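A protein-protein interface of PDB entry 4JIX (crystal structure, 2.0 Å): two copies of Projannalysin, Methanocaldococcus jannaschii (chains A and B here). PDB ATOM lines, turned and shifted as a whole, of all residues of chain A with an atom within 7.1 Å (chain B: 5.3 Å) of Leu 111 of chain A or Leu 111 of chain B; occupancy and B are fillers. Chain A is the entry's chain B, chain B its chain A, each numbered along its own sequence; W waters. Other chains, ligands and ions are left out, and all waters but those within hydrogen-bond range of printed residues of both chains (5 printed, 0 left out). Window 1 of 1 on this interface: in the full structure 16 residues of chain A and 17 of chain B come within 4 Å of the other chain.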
ATOM      1  N   MET A  36      20.007  14.939  -1.187  1.00  0.00           N
ATOM      2  CA  MET A  36      21.227  14.162  -0.985  1.00  0.00           C
ATOM      3  C   MET A  36      21.124  12.901  -1.832  1.00  0.00           C
ATOM      4  O   MET A  36      20.189  12.126  -1.651  1.00  0.00           O
ATOM      5  CB  MET A  36      21.414  13.832   0.516  1.00  0.00           C
ATOM      6  CG  MET A  36      21.692  15.042   1.399  1.00  0.00           C
ATOM      7  SD  MET A  36      21.710  14.677   3.182  1.00  0.00           S
ATOM      8  CE  MET A  36      23.347  13.982   3.358  1.00  0.00           C
ATOM      9  N   LYS A  37      22.044  12.715  -2.786  1.00  0.00           N
ATOM     10  CA  LYS A  37      22.001  11.559  -3.684  1.00  0.00           C
ATOM     11  C   LYS A  37      22.663  10.299  -3.077  1.00  0.00           C
ATOM     12  O   LYS A  37      22.364   9.189  -3.522  1.00  0.00           O
ATOM     13  CB  LYS A  37      22.648  11.898  -5.052  1.00  0.00           C
ATOM     14  CG  LYS A  37      24.098  12.379  -4.977  1.00  0.00           C
ATOM     15  CD  LYS A  37      24.702  12.604  -6.348  1.00  0.00           C
ATOM     16  CE  LYS A  37      26.175  12.921  -6.261  1.00  0.00           C
ATOM     17  NZ  LYS A  37      26.770  13.140  -7.606  1.00  0.00           N
ATOM     18  N   GLN A  38      23.528  10.470  -2.061  1.00  0.00           N
ATOM     19  CA  GLN A  38      24.311   9.378  -1.469  1.00  0.00           C
ATOM     20  C   GLN A  38      23.901   8.965  -0.046  1.00  0.00           C
ATOM     21  O   GLN A  38      24.323   7.898   0.402  1.00  0.00           O
ATOM     22  CB  GLN A  38      25.802   9.772  -1.439  1.00  0.00           C
ATOM     23  CG  GLN A  38      26.345  10.267  -2.790  1.00  0.00           C
ATOM     24  CD  GLN A  38      27.827  10.567  -2.803  1.00  0.00           C
ATOM     25  OE1 GLN A  38      28.428  10.975  -1.800  1.00  0.00           O
ATOM     26  NE2 GLN A  38      28.443  10.423  -3.971  1.00  0.00           N
ATOM     27  N   LYS A  39      23.135   9.792   0.684  1.00  0.00           N
ATOM     28  CA  LYS A  39      22.809   9.449   2.073  1.00  0.00           C
ATOM     29  C   LYS A  39      21.449   9.984   2.516  1.00  0.00           C
ATOM     30  O   LYS A  39      20.840  10.793   1.819  1.00  0.00           O
ATOM     31  CB  LYS A  39      23.924   9.997   2.998  1.00  0.00           C
ATOM     32  CG  LYS A  39      24.922   8.898   3.402  1.00  0.00           C
ATOM     33  CD  LYS A  39      26.269   9.427   3.820  1.00  0.00           C
ATOM     34  CE  LYS A  39      27.411   8.571   3.308  1.00  0.00           C
ATOM     35  NZ  LYS A  39      27.478   7.230   3.951  1.00  0.00           N
ATOM     36  N   ILE A  40      20.965   9.503   3.667  1.00  0.00           N
ATOM     37  CA  ILE A  40      19.724   9.962   4.314  1.00  0.00           C
ATOM     38  C   ILE A  40      20.098  11.069   5.317  1.00  0.00           C
ATOM     39  O   ILE A  40      19.361  12.044   5.493  1.00  0.00           O
ATOM     40  CB  ILE A  40      18.967   8.785   5.004  1.00  0.00           C
ATOM     41  CG1 ILE A  40      18.264   7.900   3.957  1.00  0.00           C
ATOM     42  CG2 ILE A  40      17.967   9.284   6.106  1.00  0.00           C
ATOM     43  CD1 ILE A  40      17.803   6.574   4.524  1.00  0.00           C
ATOM     44  N   ALA A  41      21.230  10.879   6.007  1.00  0.00           N
ATOM     45  CA  ALA A  41      21.724  11.825   7.015  1.00  0.00           C
ATOM     46  C   ALA A  41      23.201  11.618   7.241  1.00  0.00           C
ATOM     47  O   ALA A  41      23.706  10.507   7.059  1.00  0.00           O
ATOM     48  CB  ALA A  41      20.969  11.654   8.332  1.00  0.00           C
ATOM     49  N   SER A  42      23.900  12.696   7.614  1.00  0.00           N
ATOM     50  CA  SER A  42      25.328  12.645   7.929  1.00  0.00           C
ATOM     51  C   SER A  42      25.684  13.717   8.953  1.00  0.00           C
ATOM     52  O   SER A  42      24.955  14.706   9.108  1.00  0.00           O
ATOM     53  CB  SER A  42      26.181  12.807   6.674  1.00  0.00           C
ATOM     54  OG  SER A  42      25.938  14.068   6.071  1.00  0.00           O
ATOM     55  N   VAL A  56      13.498  12.776   2.638  1.00  0.00           N
ATOM     56  CA  VAL A  56      13.247  11.991   3.863  1.00  0.00           C
ATOM     57  C   VAL A  56      12.524  12.874   4.908  1.00  0.00           C
ATOM     58  O   VAL A  56      11.500  12.458   5.455  1.00  0.00           O
ATOM     59  CB  VAL A  56      14.572  11.385   4.411  1.00  0.00           C
ATOM     60  CG1 VAL A  56      14.409  10.843   5.840  1.00  0.00           C
ATOM     61  CG2 VAL A  56      15.100  10.296   3.472  1.00  0.00           C
ATOM     62  N   PHE A  60       9.132  11.047   5.556  1.00  0.00           N
ATOM     63  CA  PHE A  60       9.180  10.010   6.602  1.00  0.00           C
ATOM     64  C   PHE A  60       8.412  10.435   7.838  1.00  0.00           C
ATOM     65  O   PHE A  60       8.458  11.606   8.215  1.00  0.00           O
ATOM     66  CB  PHE A  60      10.630   9.675   6.996  1.00  0.00           C
ATOM     67  CG  PHE A  60      11.404   8.735   6.091  1.00  0.00           C
ATOM     68  CD1 PHE A  60      12.391   7.903   6.610  1.00  0.00           C
ATOM     69  CD2 PHE A  60      11.185   8.724   4.713  1.00  0.00           C
ATOM     70  CE1 PHE A  60      13.137   7.069   5.773  1.00  0.00           C
ATOM     71  CE2 PHE A  60      11.933   7.890   3.878  1.00  0.00           C
ATOM     72  CZ  PHE A  60      12.891   7.056   4.419  1.00  0.00           C
ATOM     73  N   ILE A  68      16.612   8.798  13.262  1.00  0.00           N
ATOM     74  CA  ILE A  68      17.684   9.179  12.337  1.00  0.00           C
ATOM     75  C   ILE A  68      18.533  10.326  12.930  1.00  0.00           C
ATOM     76  O   ILE A  68      19.763  10.287  12.848  1.00  0.00           O
ATOM     77  CB  ILE A  68      17.068   9.544  10.955  1.00  0.00           C
ATOM     78  CG1 ILE A  68      16.595   8.242  10.216  1.00  0.00           C
ATOM     79  CG2 ILE A  68      18.063  10.334  10.073  1.00  0.00           C
ATOM     80  CD1 ILE A  68      15.539   8.516   9.128  1.00  0.00           C
ATOM     81  N   GLU A  72      22.805  10.371  14.494  1.00  0.00           N
ATOM     82  CA  GLU A  72      23.874  11.333  14.200  1.00  0.00           C
ATOM     83  C   GLU A  72      24.316  12.118  15.411  1.00  0.00           C
ATOM     84  O   GLU A  72      25.513  12.345  15.593  1.00  0.00           O
ATOM     85  CB  GLU A  72      23.421  12.355  13.133  1.00  0.00           C
ATOM     86  CG  GLU A  72      22.853  11.796  11.832  1.00  0.00           C
ATOM     87  CD  GLU A  72      23.686  10.778  11.088  1.00  0.00           C
ATOM     88  OE1 GLU A  72      24.933  10.782  11.222  1.00  0.00           O
ATOM     89  OE2 GLU A  72      23.071   9.941  10.392  1.00  0.00           O
ATOM     90  N   GLU A 104      13.634   0.288  12.682  1.00  0.00           N
ATOM     91  CA  GLU A 104      14.597  -0.164  11.667  1.00  0.00           C
ATOM     92  C   GLU A 104      13.901  -0.906  10.537  1.00  0.00           C
ATOM     93  O   GLU A 104      14.251  -0.688   9.388  1.00  0.00           O
ATOM     94  CB  GLU A 104      15.707  -1.023  12.283  1.00  0.00           C
ATOM     95  CG  GLU A 104      16.686  -0.167  13.066  1.00  0.00           C
ATOM     96  CD  GLU A 104      17.450  -0.851  14.188  1.00  0.00           C
ATOM     97  OE1 GLU A 104      17.445  -2.102  14.265  1.00  0.00           O
ATOM     98  OE2 GLU A 104      18.083  -0.122  14.983  1.00  0.00           O
ATOM     99  N   LEU A 105      12.887  -1.722  10.852  1.00  0.00           N
ATOM    100  CA  LEU A 105      12.105  -2.432   9.837  1.00  0.00           C
ATOM    101  C   LEU A 105      11.287  -1.425   8.999  1.00  0.00           C
ATOM    102  O   LEU A 105      11.181  -1.582   7.787  1.00  0.00           O
ATOM    103  CB  LEU A 105      11.183  -3.485  10.485  1.00  0.00           C
ATOM    104  CG  LEU A 105      10.473  -4.466   9.523  1.00  0.00           C
ATOM    105  CD1 LEU A 105      11.482  -5.368   8.781  1.00  0.00           C
ATOM    106  CD2 LEU A 105       9.430  -5.311  10.263  1.00  0.00           C
ATOM    107  N   LYS A 106      10.731  -0.398   9.639  1.00  0.00           N
ATOM    108  CA  LYS A 106       9.950   0.635   8.942  1.00  0.00           C
ATOM    109  C   LYS A 106      10.831   1.430   7.979  1.00  0.00           C
ATOM    110  O   LYS A 106      10.398   1.723   6.865  1.00  0.00           O
ATOM    111  CB  LYS A 106       9.254   1.565   9.936  1.00  0.00           C
ATOM    112  CG  LYS A 106       7.979   0.941  10.508  1.00  0.00           C
ATOM    113  CD  LYS A 106       7.370   1.794  11.608  1.00  0.00           C
ATOM    114  CE  LYS A 106       6.166   1.101  12.200  1.00  0.00           C
ATOM    115  NZ  LYS A 106       5.580   1.871  13.324  1.00  0.00           N
ATOM    116  N   ILE A 107      12.061   1.761   8.389  1.00  0.00           N
ATOM    117  CA  ILE A 107      13.000   2.496   7.529  1.00  0.00           C
ATOM    118  C   ILE A 107      13.342   1.633   6.280  1.00  0.00           C
ATOM    119  O   ILE A 107      13.331   2.148   5.165  1.00  0.00           O
ATOM    120  CB  ILE A 107      14.269   2.949   8.298  1.00  0.00           C
ATOM    121  CG1 ILE A 107      13.916   4.058   9.348  1.00  0.00           C
ATOM    122  CG2 ILE A 107      15.381   3.427   7.316  1.00  0.00           C
ATOM    123  CD1 ILE A 107      15.058   4.373  10.369  1.00  0.00           C
ATOM    124  N   ILE A 108      13.632   0.339   6.473  1.00  0.00           N
ATOM    125  CA  ILE A 108      13.944  -0.576   5.363  1.00  0.00           C
ATOM    126  C   ILE A 108      12.762  -0.680   4.382  1.00  0.00           C
ATOM    127  O   ILE A 108      12.970  -0.664   3.166  1.00  0.00           O
ATOM    128  CB  ILE A 108      14.353  -1.980   5.911  1.00  0.00           C
ATOM    129  CG1 ILE A 108      15.762  -1.924   6.526  1.00  0.00           C
ATOM    130  CG2 ILE A 108      14.277  -3.082   4.819  1.00  0.00           C
ATOM    131  CD1 ILE A 108      16.978  -1.706   5.488  1.00  0.00           C
ATOM    132  N   GLN A 109      11.528  -0.745   4.914  1.00  0.00           N
ATOM    133  CA  GLN A 109      10.334  -0.892   4.097  1.00  0.00           C
ATOM    134  C   GLN A 109      10.017   0.416   3.328  1.00  0.00           C
ATOM    135  O   GLN A 109       9.343   0.357   2.306  1.00  0.00           O
ATOM    136  CB  GLN A 109       9.169  -1.402   4.942  1.00  0.00           C
ATOM    137  CG  GLN A 109       9.382  -2.872   5.366  1.00  0.00           C
ATOM    138  CD  GLN A 109       8.306  -3.433   6.273  1.00  0.00           C
ATOM    139  OE1 GLN A 109       7.533  -2.703   6.908  1.00  0.00           O
ATOM    140  NE2 GLN A 109       8.270  -4.759   6.394  1.00  0.00           N
ATOM    141  N   LYS A 110      10.594   1.551   3.748  1.00  0.00           N
ATOM    142  CA  LYS A 110      10.516   2.836   3.041  1.00  0.00           C
ATOM    143  C   LYS A 110      11.585   2.890   1.912  1.00  0.00           C
ATOM    144  O   LYS A 110      11.410   3.611   0.932  1.00  0.00           O
ATOM    145  CB  LYS A 110      10.743   3.992   4.035  1.00  0.00           C
ATOM    146  CG  LYS A 110       9.734   5.121   3.924  1.00  0.00           C
ATOM    147  CD  LYS A 110       8.424   4.865   4.636  1.00  0.00           C
ATOM    148  CE  LYS A 110       7.552   6.097   4.593  1.00  0.00           C
ATOM    149  NZ  LYS A 110       7.026   6.378   3.227  1.00  0.00           N
ATOM    150  N   LEU A 111      12.684   2.118   2.046  1.00  0.00           N
ATOM    151  CA  LEU A 111      13.792   2.135   1.072  1.00  0.00           C
ATOM    152  C   LEU A 111      13.697   1.081  -0.014  1.00  0.00           C
ATOM    153  O   LEU A 111      14.150   1.329  -1.129  1.00  0.00           O
ATOM    154  CB  LEU A 111      15.135   1.945   1.801  1.00  0.00           C
ATOM    155  CG  LEU A 111      15.536   3.042   2.792  1.00  0.00           C
ATOM    156  CD1 LEU A 111      16.716   2.598   3.630  1.00  0.00           C
ATOM    157  CD2 LEU A 111      15.778   4.357   2.104  1.00  0.00           C
ATOM    158  N   ILE A 112      13.192  -0.121   0.315  1.00  0.00           N
ATOM    159  CA  ILE A 112      13.122  -1.230  -0.643  1.00  0.00           C
ATOM    160  C   ILE A 112      11.710  -1.834  -0.687  1.00  0.00           C
ATOM    161  O   ILE A 112      11.409  -2.543  -1.676  1.00  0.00           O
ATOM    162  CB  ILE A 112      14.210  -2.313  -0.322  1.00  0.00           C
ATOM    163  CG1 ILE A 112      13.894  -3.106   0.970  1.00  0.00           C
ATOM    164  CG2 ILE A 112      15.616  -1.682  -0.254  1.00  0.00           C
ATOM    165  CD1 ILE A 112      14.883  -4.296   1.281  1.00  0.00           C
ATOM    166  OXT ILE A 112      10.913  -1.589   0.252  1.00  0.00           O
ATOM    167  N   LYS B  39      13.696   6.042  -3.270  1.00  0.00           N
ATOM    168  CA  LYS B  39      14.002   4.662  -2.845  1.00  0.00           C
ATOM    169  C   LYS B  39      15.399   4.248  -3.260  1.00  0.00           C
ATOM    170  O   LYS B  39      16.028   4.902  -4.102  1.00  0.00           O
ATOM    171  CB  LYS B  39      13.021   3.649  -3.518  1.00  0.00           C
ATOM    172  CG  LYS B  39      11.524   3.938  -3.444  1.00  0.00           C
ATOM    173  CD  LYS B  39      10.870   3.266  -2.269  1.00  0.00           C
ATOM    174  CE  LYS B  39       9.492   3.824  -2.021  1.00  0.00           C
ATOM    175  NZ  LYS B  39       9.006   3.514  -0.648  1.00  0.00           N
ATOM    176  N   ILE B  40      15.848   3.093  -2.756  1.00  0.00           N
ATOM    177  CA  ILE B  40      17.107   2.538  -3.220  1.00  0.00           C
ATOM    178  C   ILE B  40      16.767   1.367  -4.186  1.00  0.00           C
ATOM    179  O   ILE B  40      17.584   1.017  -5.030  1.00  0.00           O
ATOM    180  CB  ILE B  40      18.114   2.183  -2.100  1.00  0.00           C
ATOM    181  CG1 ILE B  40      17.622   1.051  -1.197  1.00  0.00           C
ATOM    182  CG2 ILE B  40      18.487   3.459  -1.297  1.00  0.00           C
ATOM    183  CD1 ILE B  40      18.692   0.572  -0.065  1.00  0.00           C
ATOM    184  N   ALA B  41      15.539   0.815  -4.089  1.00  0.00           N
ATOM    185  CA  ALA B  41      15.072  -0.248  -4.979  1.00  0.00           C
ATOM    186  C   ALA B  41      13.552  -0.331  -5.014  1.00  0.00           C
ATOM    187  O   ALA B  41      12.872  -0.028  -4.036  1.00  0.00           O
ATOM    188  CB  ALA B  41      15.652  -1.597  -4.570  1.00  0.00           C
ATOM    189  N   VAL B  56      23.879   3.308  -5.082  1.00  0.00           N
ATOM    190  CA  VAL B  56      23.837   2.079  -4.281  1.00  0.00           C
ATOM    191  C   VAL B  56      24.484   0.927  -5.075  1.00  0.00           C
ATOM    192  O   VAL B  56      25.336   0.229  -4.537  1.00  0.00           O
ATOM    193  CB  VAL B  56      22.365   1.774  -3.869  1.00  0.00           C
ATOM    194  CG1 VAL B  56      22.198   0.358  -3.322  1.00  0.00           C
ATOM    195  CG2 VAL B  56      21.868   2.801  -2.855  1.00  0.00           C
ATOM    196  N   PHE B  60      27.586  -0.187  -2.846  1.00  0.00           N
ATOM    197  CA  PHE B  60      27.274  -1.184  -1.807  1.00  0.00           C
ATOM    198  C   PHE B  60      27.941  -2.514  -2.105  1.00  0.00           C
ATOM    199  O   PHE B  60      28.034  -2.895  -3.271  1.00  0.00           O
ATOM    200  CB  PHE B  60      25.754  -1.402  -1.685  1.00  0.00           C
ATOM    201  CG  PHE B  60      24.961  -0.427  -0.839  1.00  0.00           C
ATOM    202  CD1 PHE B  60      23.782  -0.823  -0.222  1.00  0.00           C
ATOM    203  CD2 PHE B  60      25.363   0.900  -0.707  1.00  0.00           C
ATOM    204  CE1 PHE B  60      23.035   0.080   0.539  1.00  0.00           C
ATOM    205  CE2 PHE B  60      24.603   1.807   0.035  1.00  0.00           C
ATOM    206  CZ  PHE B  60      23.446   1.391   0.652  1.00  0.00           C
ATOM    207  N   ILE B 107      22.558  -1.884   5.818  1.00  0.00           N
ATOM    208  CA  ILE B 107      21.955  -1.026   4.789  1.00  0.00           C
ATOM    209  C   ILE B 107      21.635   0.346   5.401  1.00  0.00           C
ATOM    210  O   ILE B 107      22.035   1.386   4.864  1.00  0.00           O
ATOM    211  CB  ILE B 107      20.709  -1.697   4.160  1.00  0.00           C
ATOM    212  CG1 ILE B 107      21.139  -2.959   3.339  1.00  0.00           C
ATOM    213  CG2 ILE B 107      19.906  -0.678   3.280  1.00  0.00           C
ATOM    214  CD1 ILE B 107      19.953  -3.942   2.966  1.00  0.00           C
ATOM    215  N   ILE B 108      20.939   0.348   6.537  1.00  0.00           N
ATOM    216  CA  ILE B 108      20.571   1.604   7.209  1.00  0.00           C
ATOM    217  C   ILE B 108      21.830   2.433   7.509  1.00  0.00           C
ATOM    218  O   ILE B 108      21.858   3.630   7.215  1.00  0.00           O
ATOM    219  CB  ILE B 108      19.745   1.308   8.505  1.00  0.00           C
ATOM    220  CG1 ILE B 108      18.346   0.754   8.130  1.00  0.00           C
ATOM    221  CG2 ILE B 108      19.603   2.573   9.383  1.00  0.00           C
ATOM    222  CD1 ILE B 108      17.596   0.046   9.231  1.00  0.00           C
ATOM    223  N   GLN B 109      22.877   1.786   8.046  1.00  0.00           N
ATOM    224  CA  GLN B 109      24.093   2.475   8.472  1.00  0.00           C
ATOM    225  C   GLN B 109      25.026   2.845   7.305  1.00  0.00           C
ATOM    226  O   GLN B 109      25.966   3.612   7.505  1.00  0.00           O
ATOM    227  CB  GLN B 109      24.797   1.721   9.606  1.00  0.00           C
ATOM    228  CG  GLN B 109      23.848   1.756  10.841  1.00  0.00           C
ATOM    229  CD  GLN B 109      24.318   1.140  12.147  1.00  0.00           C
ATOM    230  OE1 GLN B 109      23.757   1.429  13.208  1.00  0.00           O
ATOM    231  NE2 GLN B 109      25.303   0.256  12.117  1.00  0.00           N
ATOM    232  N   LYS B 110      24.680   2.451   6.079  1.00  0.00           N
ATOM    233  CA  LYS B 110      25.367   2.951   4.885  1.00  0.00           C
ATOM    234  C   LYS B 110      24.773   4.322   4.524  1.00  0.00           C
ATOM    235  O   LYS B 110      25.377   5.073   3.761  1.00  0.00           O
ATOM    236  CB  LYS B 110      25.185   1.974   3.689  1.00  0.00           C
ATOM    237  CG  LYS B 110      26.113   0.755   3.704  1.00  0.00           C
ATOM    238  CD  LYS B 110      27.594   1.076   3.574  1.00  0.00           C
ATOM    239  CE  LYS B 110      28.013   1.443   2.172  1.00  0.00           C
ATOM    240  NZ  LYS B 110      29.441   1.860   2.134  1.00  0.00           N
ATOM    241  N   LEU B 111      23.554   4.626   5.041  1.00  0.00           N
ATOM    242  CA  LEU B 111      22.825   5.842   4.672  1.00  0.00           C
ATOM    243  C   LEU B 111      22.680   6.856   5.793  1.00  0.00           C
ATOM    244  O   LEU B 111      22.388   8.023   5.511  1.00  0.00           O
ATOM    245  CB  LEU B 111      21.434   5.452   4.143  1.00  0.00           C
ATOM    246  CG  LEU B 111      21.468   4.433   2.976  1.00  0.00           C
ATOM    247  CD1 LEU B 111      20.123   3.779   2.795  1.00  0.00           C
ATOM    248  CD2 LEU B 111      21.922   5.088   1.694  1.00  0.00           C
ATOM    249  N   ILE B 112      22.884   6.427   7.051  1.00  0.00           N
ATOM    250  CA  ILE B 112      22.853   7.304   8.239  1.00  0.00           C
ATOM    251  C   ILE B 112      24.123   7.044   9.058  1.00  0.00           C
ATOM    252  O   ILE B 112      24.519   7.927   9.847  1.00  0.00           O
ATOM    253  CB  ILE B 112      21.559   7.166   9.102  1.00  0.00           C
ATOM    254  CG1 ILE B 112      21.472   5.804   9.844  1.00  0.00           C
ATOM    255  CG2 ILE B 112      20.294   7.455   8.276  1.00  0.00           C
ATOM    256  CD1 ILE B 112      20.442   5.790  11.026  1.00  0.00           C
ATOM    257  OXT ILE B 112      24.704   5.943   8.934  1.00  0.00           O
HETATM  258  O   HOH W   1      26.486   6.473   6.774  1.00  0.00           O
HETATM  259  O   HOH W   2      26.168   9.160   7.328  1.00  0.00           O
HETATM  260  O   HOH W   3      10.339  -0.086  -3.344  1.00  0.00           O
HETATM  261  O   HOH W   4      25.864   5.400   0.886  1.00  0.00           O
HETATM  262  O   HOH W   5       9.816   0.898  -0.735  1.00  0.00           O
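Lys 39 of chain A touches Leu 111 of chain B, and with the chains exchanged Leu 111 of chain A touches Lys 39 of chain B.
Ile 40 of chain A touches Ile 112 of chain B, and with the chains exchanged Ile 112 of chain A touches Ile 40 of chain B.
Ile 108 of chain B touches its own counterpart, Ile 108 of chain A.
Leu 111 of chain B touches its own counterpart, Leu 111 of chain A.
Of chain B, only Lys 39 (3.5 Å), Ile 40 (2.9 Å), Ala 41 (3.3 Å) and Leu 111 (3.7 Å) come within 4 Å of Leu 111 of chain A.
Printed residues of chain A within 4 Å of Ile 107 of chain B: Ile 108.
Printed residues of chain A within 4 Å of Ile 40 of chain B: Leu 111 and Ile 112.
Of the printed residues of chain B, Gln 38 of chain A touches Leu 111 (3.9 Å).
Of the printed residues of chain B, Ile 112 of chain A touches Ile 40 (3.5 Å) and Ala 41 (3.6 Å).
The nearest residue of chain B that does not touch Leu 111 of chain A is Ile 107 of chain B (4.6 Å).
The nearest residue of chain A that does not touch Leu 111 of chain B is Glu 72 of chain A (5.3 Å).
The nearest printed residue of chain B that does not touch Glu 104 of chain A is Gln 109 of chain B (6.1 Å).
The side-chain amino group (NZ) of Lys 39 of chain B lies within hydrogen-bond range of the backbone carbonyl oxygen (O) of Lys 110 of chain A (2.9 Å).
The backbone carbonyl oxygen (O) of Leu 111 of chain A lies within hydrogen-bond range of the backbone NH (N) of Ile 40 of chain B (2.9 Å).
N of Ala 41 of chain B sits at hydrogen-bond distance from O of Leu 111 of chain A, at 3.3 Å.
The backbone carbonyl oxygen (O) of Lys 110 of chain B sits at hydrogen-bond distance from the side-chain amino group (NZ) of Lys 39 of chain A.
The backbone NH (N) of Ile 40 of chain A lies within hydrogen-bond range of the backbone carbonyl oxygen (O) of Leu 111 of chain B, at 2.8 Å.
O of Leu 111 of chain B sits at hydrogen-bond distance from N of Ala 41 of chain A (3.1 Å).
O of Ile 112 of chain B sits close to OE2 of Glu 72 of chain A (2.5 Å).
Of the 20 printed residues of chain A, 10 touch a printed residue of chain B.
Among the printed residues, no Asp or Glu carboxylate lies within 4 Å of a Lys or Arg side-chain nitrogen of the other chain.
O of Gln 38 of chain A touches CD2 of Leu 111 of chain B, 3.9 Å away.
Leu 111 of chain B touches Lys 39 of chain A.
Ile 40 of chain A touches Ile 112 of chain B.
Ile 108 of chain B touches Glu 104 of chain A.
CG2 of Ile 107 of chain B touches CD1 of Ile 108 of chain A, 3.8 Å away.
Ile 108 of chain B touches Ile 108 of chain A.
Lys 39 of chain B touches Leu 111 of chain A.
CD1 of Leu 111 of chain A touches CD1 of Leu 111 of chain B (3.7 Å).
Ile 112 of chain A touches Ile 40 of chain B.
CA of Ile 112 of chain A touches O of Ala 41 of chain B (3.6 Å).
Water W3 bridges the backbone carbonyl oxygen (O) of Ala 41 of chain B and the chain-end carboxylate (O) of Ile 112 of chain A.
Water W5 lies within hydrogen-bond range of the side-chain amino group (NZ) of Lys 39 of chain B, the chain-end carboxylate (OXT) of Ile 112 of chain A and the backbone carbonyl oxygen (O) of Gln 109 of chain A.
Water W2 lies within hydrogen-bond range of O of Ala 41 of chain A and O of Ile 112 of chain B.
Water W1 lies within hydrogen-bond range of the chain-end carboxylate of Ile 112 of chain B (2.8 Å), the backbone carbonyl oxygen of Gln 109 of chain B (3.0 Å) and the side-chain amino group of Lys 39 of chain A (3.1 Å).
Water W4 lies within hydrogen-bond range of the backbone carbonyl oxygen of Lys 110 of chain B (2.9 Å) and the backbone carbonyl oxygen of Gln 38 of chain A (3.0 Å).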
